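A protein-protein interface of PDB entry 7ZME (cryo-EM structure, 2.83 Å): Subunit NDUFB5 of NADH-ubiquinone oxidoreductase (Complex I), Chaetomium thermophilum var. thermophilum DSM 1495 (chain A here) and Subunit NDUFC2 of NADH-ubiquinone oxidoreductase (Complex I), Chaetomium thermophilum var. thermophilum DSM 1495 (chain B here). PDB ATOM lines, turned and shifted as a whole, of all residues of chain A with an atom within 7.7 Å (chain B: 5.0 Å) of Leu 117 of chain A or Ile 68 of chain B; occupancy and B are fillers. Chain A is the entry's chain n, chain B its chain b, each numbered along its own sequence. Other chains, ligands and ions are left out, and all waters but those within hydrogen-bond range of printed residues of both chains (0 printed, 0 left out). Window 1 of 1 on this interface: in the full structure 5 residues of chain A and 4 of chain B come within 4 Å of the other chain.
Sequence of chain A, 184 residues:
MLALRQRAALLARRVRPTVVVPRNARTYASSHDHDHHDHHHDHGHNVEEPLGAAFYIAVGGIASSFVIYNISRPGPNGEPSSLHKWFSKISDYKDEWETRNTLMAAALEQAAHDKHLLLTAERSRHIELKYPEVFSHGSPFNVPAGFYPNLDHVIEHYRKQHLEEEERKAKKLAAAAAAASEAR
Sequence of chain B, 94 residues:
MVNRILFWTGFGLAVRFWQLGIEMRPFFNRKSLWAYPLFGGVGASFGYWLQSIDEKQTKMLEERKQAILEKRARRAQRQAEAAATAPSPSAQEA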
ATOM      1  N   ALA A 111       5.722   0.082   3.325  1.00  0.00           N
ATOM      2  CA  ALA A 111       5.101  -0.275   4.619  1.00  0.00           C
ATOM      3  C   ALA A 111       6.062   0.119   5.736  1.00  0.00           C
ATOM      4  O   ALA A 111       5.627   0.793   6.679  1.00  0.00           O
ATOM      5  CB  ALA A 111       4.804  -1.746   4.649  1.00  0.00           C
ATOM      6  N   ALA A 112       7.320  -0.317   5.630  1.00  0.00           N
ATOM      7  CA  ALA A 112       8.319  -0.084   6.698  1.00  0.00           C
ATOM      8  C   ALA A 112       8.562   1.411   6.916  1.00  0.00           C
ATOM      9  O   ALA A 112       8.697   1.812   8.079  1.00  0.00           O
ATOM     10  CB  ALA A 112       9.597  -0.807   6.365  1.00  0.00           C
ATOM     11  N   HIS A 113       8.616   2.192   5.840  1.00  0.00           N
ATOM     12  CA  HIS A 113       8.820   3.652   5.970  1.00  0.00           C
ATOM     13  C   HIS A 113       7.650   4.243   6.753  1.00  0.00           C
ATOM     14  O   HIS A 113       7.899   5.055   7.652  1.00  0.00           O
ATOM     15  CB  HIS A 113       8.946   4.277   4.577  1.00  0.00           C
ATOM     16  CG  HIS A 113       9.029   5.767   4.587  1.00  0.00           C
ATOM     17  ND1 HIS A 113      10.231   6.438   4.504  1.00  0.00           N
ATOM     18  CD2 HIS A 113       8.071   6.715   4.672  1.00  0.00           C
ATOM     19  CE1 HIS A 113      10.011   7.735   4.540  1.00  0.00           C
ATOM     20  NE2 HIS A 113       8.694   7.931   4.645  1.00  0.00           N
ATOM     21  N   ASP A 114       6.431   3.822   6.431  1.00  0.00           N
ATOM     22  CA  ASP A 114       5.219   4.342   7.113  1.00  0.00           C
ATOM     23  C   ASP A 114       5.260   3.951   8.584  1.00  0.00           C
ATOM     24  O   ASP A 114       4.991   4.815   9.432  1.00  0.00           O
ATOM     25  CB  ASP A 114       3.958   3.772   6.470  1.00  0.00           C
ATOM     26  CG  ASP A 114       3.801   4.157   5.010  1.00  0.00           C
ATOM     27  OD1 ASP A 114       4.519   5.075   4.565  1.00  0.00           O
ATOM     28  OD2 ASP A 114       2.967   3.532   4.326  1.00  0.00           O
ATOM     29  N   LYS A 115       5.620   2.701   8.862  1.00  0.00           N
ATOM     30  CA  LYS A 115       5.634   2.206  10.256  1.00  0.00           C
ATOM     31  C   LYS A 115       6.670   3.010  11.016  1.00  0.00           C
ATOM     32  O   LYS A 115       6.387   3.421  12.147  1.00  0.00           O
ATOM     33  CB  LYS A 115       5.997   0.719  10.258  1.00  0.00           C
ATOM     34  CG  LYS A 115       5.943   0.024  11.611  1.00  0.00           C
ATOM     35  CD  LYS A 115       6.368  -1.429  11.545  1.00  0.00           C
ATOM     36  CE  LYS A 115       6.170  -2.164  12.853  1.00  0.00           C
ATOM     37  NZ  LYS A 115       6.933  -1.536  13.956  1.00  0.00           N
ATOM     38  N   HIS A 116       7.817   3.244  10.386  1.00  0.00           N
ATOM     39  CA  HIS A 116       8.916   3.989  11.048  1.00  0.00           C
ATOM     40  C   HIS A 116       8.446   5.410  11.348  1.00  0.00           C
ATOM     41  O   HIS A 116       8.549   5.811  12.497  1.00  0.00           O
ATOM     42  CB  HIS A 116      10.156   3.866  10.167  1.00  0.00           C
ATOM     43  CG  HIS A 116      11.247   4.835  10.442  1.00  0.00           C
ATOM     44  ND1 HIS A 116      12.186   5.159   9.489  1.00  0.00           N
ATOM     45  CD2 HIS A 116      11.566   5.538  11.543  1.00  0.00           C
ATOM     46  CE1 HIS A 116      13.024   6.035   9.985  1.00  0.00           C
ATOM     47  NE2 HIS A 116      12.664   6.280  11.242  1.00  0.00           N
ATOM     48  N   LEU A 117       7.801   6.062  10.390  1.00  0.00           N
ATOM     49  CA  LEU A 117       7.325   7.451  10.568  1.00  0.00           C
ATOM     50  C   LEU A 117       6.297   7.514  11.705  1.00  0.00           C
ATOM     51  O   LEU A 117       6.317   8.504  12.453  1.00  0.00           O
ATOM     52  CB  LEU A 117       6.735   7.897   9.228  1.00  0.00           C
ATOM     53  CG  LEU A 117       6.277   9.349   9.149  1.00  0.00           C
ATOM     54  CD1 LEU A 117       7.471  10.276   9.005  1.00  0.00           C
ATOM     55  CD2 LEU A 117       5.317   9.536   7.989  1.00  0.00           C
ATOM     56  N   LEU A 118       5.429   6.506  11.824  1.00  0.00           N
ATOM     57  CA  LEU A 118       4.375   6.482  12.869  1.00  0.00           C
ATOM     58  C   LEU A 118       4.950   6.176  14.265  1.00  0.00           C
ATOM     59  O   LEU A 118       4.569   6.901  15.194  1.00  0.00           O
ATOM     60  CB  LEU A 118       3.280   5.490  12.466  1.00  0.00           C
ATOM     61  CG  LEU A 118       2.412   5.885  11.272  1.00  0.00           C
ATOM     62  CD1 LEU A 118       1.735   4.665  10.672  1.00  0.00           C
ATOM     63  CD2 LEU A 118       1.378   6.924  11.667  1.00  0.00           C
ATOM     64  N   LEU A 119       5.800   5.155  14.436  1.00  0.00           N
ATOM     65  CA  LEU A 119       6.285   4.853  15.778  1.00  0.00           C
ATOM     66  C   LEU A 119       7.354   5.823  16.255  1.00  0.00           C
ATOM     67  O   LEU A 119       7.556   5.950  17.465  1.00  0.00           O
ATOM     68  CB  LEU A 119       6.809   3.418  15.858  1.00  0.00           C
ATOM     69  CG  LEU A 119       5.784   2.284  15.966  1.00  0.00           C
ATOM     70  CD1 LEU A 119       5.010   2.044  14.684  1.00  0.00           C
ATOM     71  CD2 LEU A 119       6.489   1.013  16.404  1.00  0.00           C
ATOM     72  N   THR A 120       8.038   6.509  15.346  1.00  0.00           N
ATOM     73  CA  THR A 120       9.033   7.501  15.719  1.00  0.00           C
ATOM     74  C   THR A 120       8.457   8.905  15.772  1.00  0.00           C
ATOM     75  O   THR A 120       9.217   9.867  15.916  1.00  0.00           O
ATOM     76  CB  THR A 120      10.215   7.464  14.754  1.00  0.00           C
ATOM     77  OG1 THR A 120       9.754   7.734  13.426  1.00  0.00           O
ATOM     78  CG2 THR A 120      10.891   6.105  14.785  1.00  0.00           C
ATOM     79  N   ALA A 121       7.139   9.043  15.647  1.00  0.00           N
ATOM     80  CA  ALA A 121       6.514  10.358  15.694  1.00  0.00           C
ATOM     81  C   ALA A 121       6.787  11.027  17.031  1.00  0.00           C
ATOM     82  O   ALA A 121       6.740  10.390  18.085  1.00  0.00           O
ATOM     83  CB  ALA A 121       5.009  10.241  15.457  1.00  0.00           C
ATOM     84  N   GLU A 122       7.091  12.318  16.977  1.00  0.00           N
ATOM     85  CA  GLU A 122       7.464  13.056  18.175  1.00  0.00           C
ATOM     86  C   GLU A 122       6.293  13.133  19.143  1.00  0.00           C
ATOM     87  O   GLU A 122       5.152  13.381  18.742  1.00  0.00           O
ATOM     88  CB  GLU A 122       7.938  14.457  17.801  1.00  0.00           C
ATOM     89  CG  GLU A 122       8.720  14.510  16.498  1.00  0.00           C
ATOM     90  CD  GLU A 122       9.353  15.864  16.249  1.00  0.00           C
ATOM     91  OE1 GLU A 122       8.834  16.870  16.775  1.00  0.00           O
ATOM     92  OE2 GLU A 122      10.370  15.920  15.527  1.00  0.00           O
ATOM     93  N   ARG B  64      -2.712  11.216   8.647  1.00  0.00           N
ATOM     94  CA  ARG B  64      -1.767  11.270   9.753  1.00  0.00           C
ATOM     95  C   ARG B  64      -0.325  11.203   9.271  1.00  0.00           C
ATOM     96  O   ARG B  64       0.515  11.975   9.741  1.00  0.00           O
ATOM     97  CB  ARG B  64      -2.050  10.146  10.746  1.00  0.00           C
ATOM     98  CG  ARG B  64      -1.057  10.092  11.873  1.00  0.00           C
ATOM     99  CD  ARG B  64      -1.430  11.101  12.931  1.00  0.00           C
ATOM    100  NE  ARG B  64      -0.349  11.329  13.881  1.00  0.00           N
ATOM    101  CZ  ARG B  64       0.413  12.416  13.898  1.00  0.00           C
ATOM    102  NH1 ARG B  64       0.217  13.378  13.011  1.00  0.00           N
ATOM    103  NH2 ARG B  64       1.373  12.538  14.802  1.00  0.00           N
ATOM    104  N   LYS B  65      -0.011  10.297   8.341  1.00  0.00           N
ATOM    105  CA  LYS B  65       1.354  10.226   7.828  1.00  0.00           C
ATOM    106  C   LYS B  65       1.734  11.490   7.074  1.00  0.00           C
ATOM    107  O   LYS B  65       2.891  11.917   7.122  1.00  0.00           O
ATOM    108  CB  LYS B  65       1.545   8.999   6.934  1.00  0.00           C
ATOM    109  CG  LYS B  65       1.390   7.664   7.644  1.00  0.00           C
ATOM    110  CD  LYS B  65       1.670   6.507   6.700  1.00  0.00           C
ATOM    111  CE  LYS B  65       0.584   6.334   5.650  1.00  0.00           C
ATOM    112  NZ  LYS B  65      -0.713   5.923   6.248  1.00  0.00           N
ATOM    113  N   GLN B  66       0.780  12.098   6.369  1.00  0.00           N
ATOM    114  CA  GLN B  66       1.037  13.399   5.764  1.00  0.00           C
ATOM    115  C   GLN B  66       1.270  14.460   6.830  1.00  0.00           C
ATOM    116  O   GLN B  66       2.146  15.318   6.681  1.00  0.00           O
ATOM    117  CB  GLN B  66      -0.123  13.792   4.853  1.00  0.00           C
ATOM    118  CG  GLN B  66      -0.192  12.994   3.567  1.00  0.00           C
ATOM    119  CD  GLN B  66       1.175  12.599   3.046  1.00  0.00           C
ATOM    120  OE1 GLN B  66       1.499  11.416   2.960  1.00  0.00           O
ATOM    121  NE2 GLN B  66       1.977  13.591   2.673  1.00  0.00           N
ATOM    122  N   ALA B  67       0.496  14.412   7.916  1.00  0.00           N
ATOM    123  CA  ALA B  67       0.662  15.377   8.995  1.00  0.00           C
ATOM    124  C   ALA B  67       2.029  15.250   9.653  1.00  0.00           C
ATOM    125  O   ALA B  67       2.639  16.256  10.029  1.00  0.00           O
ATOM    126  CB  ALA B  67      -0.450  15.202  10.027  1.00  0.00           C
ATOM    127  N   ILE B  68       2.519  14.022   9.819  1.00  0.00           N
ATOM    128  CA  ILE B  68       3.826  13.828  10.438  1.00  0.00           C
ATOM    129  C   ILE B  68       4.930  14.377   9.544  1.00  0.00           C
ATOM    130  O   ILE B  68       5.840  15.067  10.016  1.00  0.00           O
ATOM    131  CB  ILE B  68       4.052  12.343  10.771  1.00  0.00           C
ATOM    132  CG1 ILE B  68       2.982  11.844  11.736  1.00  0.00           C
ATOM    133  CG2 ILE B  68       5.423  12.145  11.387  1.00  0.00           C
ATOM    134  CD1 ILE B  68       3.055  10.364  12.017  1.00  0.00           C
ATOM    135  N   LEU B  69       4.868  14.086   8.242  1.00  0.00           N
ATOM    136  CA  LEU B  69       5.869  14.603   7.315  1.00  0.00           C
ATOM    137  C   LEU B  69       5.838  16.125   7.254  1.00  0.00           C
ATOM    138  O   LEU B  69       6.891  16.773   7.244  1.00  0.00           O
ATOM    139  CB  LEU B  69       5.648  14.015   5.923  1.00  0.00           C
ATOM    140  CG  LEU B  69       5.857  12.515   5.735  1.00  0.00           C
ATOM    141  CD1 LEU B  69       5.454  12.101   4.333  1.00  0.00           C
ATOM    142  CD2 LEU B  69       7.305  12.154   6.001  1.00  0.00           C
ATOM    143  N   GLU B  70       4.641  16.711   7.206  1.00  0.00           N
ATOM    144  CA  GLU B  70       4.530  18.164   7.152  1.00  0.00           C
ATOM    145  C   GLU B  70       5.040  18.817   8.427  1.00  0.00           C
ATOM    146  O   GLU B  70       5.645  19.892   8.371  1.00  0.00           O
ATOM    147  CB  GLU B  70       3.081  18.571   6.886  1.00  0.00           C
ATOM    148  CG  GLU B  70       2.636  18.352   5.449  1.00  0.00           C
ATOM    149  CD  GLU B  70       1.215  18.816   5.200  1.00  0.00           C
ATOM    150  OE1 GLU B  70       0.517  19.148   6.180  1.00  0.00           O
ATOM    151  OE2 GLU B  70       0.798  18.852   4.022  1.00  0.00           O
ATOM    152  N   LYS B  71       4.794  18.195   9.580  1.00  0.00           N
ATOM    153  CA  LYS B  71       5.370  18.691  10.824  1.00  0.00           C
ATOM    154  C   LYS B  71       6.889  18.642  10.779  1.00  0.00           C
ATOM    155  O   LYS B  71       7.562  19.594  11.192  1.00  0.00           O
ATOM    156  CB  LYS B  71       4.843  17.874  12.001  1.00  0.00           C
ATOM    157  CG  LYS B  71       5.486  18.212  13.330  1.00  0.00           C
ATOM    158  CD  LYS B  71       4.957  19.523  13.884  1.00  0.00           C
ATOM    159  CE  LYS B  71       5.592  19.840  15.224  1.00  0.00           C
ATOM    160  NZ  LYS B  71       5.261  18.808  16.243  1.00  0.00           N
ATOM    161  N   ARG B  72       7.448  17.541  10.272  1.00  0.00           N
ATOM    162  CA  ARG B  72       8.898  17.403  10.209  1.00  0.00           C
ATOM    163  C   ARG B  72       9.496  18.302   9.137  1.00  0.00           C
ATOM    164  O   ARG B  72      10.561  18.896   9.341  1.00  0.00           O
ATOM    165  CB  ARG B  72       9.275  15.945   9.952  1.00  0.00           C
ATOM    166  CG  ARG B  72       8.805  14.974  11.025  1.00  0.00           C
ATOM    167  CD  ARG B  72       9.360  13.583  10.772  1.00  0.00           C
ATOM    168  NE  ARG B  72      10.723  13.646  10.254  1.00  0.00           N
ATOM    169  CZ  ARG B  72      11.807  13.736  11.017  1.00  0.00           C
ATOM    170  NH1 ARG B  72      11.689  13.771  12.336  1.00  0.00           N
ATOM    171  NH2 ARG B  72      13.007  13.793  10.460  1.00  0.00           N
ATOM    172  N   ALA B  73       8.835  18.400   7.981  1.00  0.00           N
ATOM    173  CA  ALA B  73       9.348  19.241   6.906  1.00  0.00           C
ATOM    174  C   ALA B  73       9.385  20.705   7.323  1.00  0.00           C
ATOM    175  O   ALA B  73      10.348  21.419   7.025  1.00  0.00           O
ATOM    176  CB  ALA B  73       8.503  19.061   5.646  1.00  0.00           C
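Among the printed residues, merely in contact across the chains: Asp 114 of chain A with Lys 65 of chain B, Leu 117 of chain A with Lys 65 of chain B, Leu 117 of chain A with Ile 68 of chain B, Leu 117 of chain A with Leu 69 of chain B, Leu 118 of chain A with Ile 68 of chain B and Ala 121 of chain A with Ile 68 of chain B.
Leu 117 of chain A touches just these residues of chain B: Lys 65, Ile 68 and Leu 69. Ile 68 of chain B touches just these residues of chain A: Leu 117, Leu 118 and Ala 121. No residue of chain A comes within 4 Å of Ala 67 of chain B. Of the printed residues of chain B, Ala 121 of chain A touches Ile 68 (3.96 Å). Of the printed residues of chain B, Leu 118 of chain A touches Ile 68 (3.8 Å). Of the printed residues of chain A, Leu 69 of chain B touches Leu 117 (3.5 Å). The nearest residue of chain A that does not touch Ile 68 of chain B is Glu 122 of chain A (5.8 Å).
Printed residues of chain B that touch a printed residue of chain A: Lys 65, Ile 68 and Leu 69. Hydrophobic or aromatic side chains of chain B that line the printed part of chain A: Ile 68 and Leu 69. Along chain B the printed residues that touch a printed residue of chain A span positions 65 to 69. Along chain A the printed residues that touch a printed residue of chain B span positions 114 to 121. Among the printed residues, 6 pairs touch across the chains.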
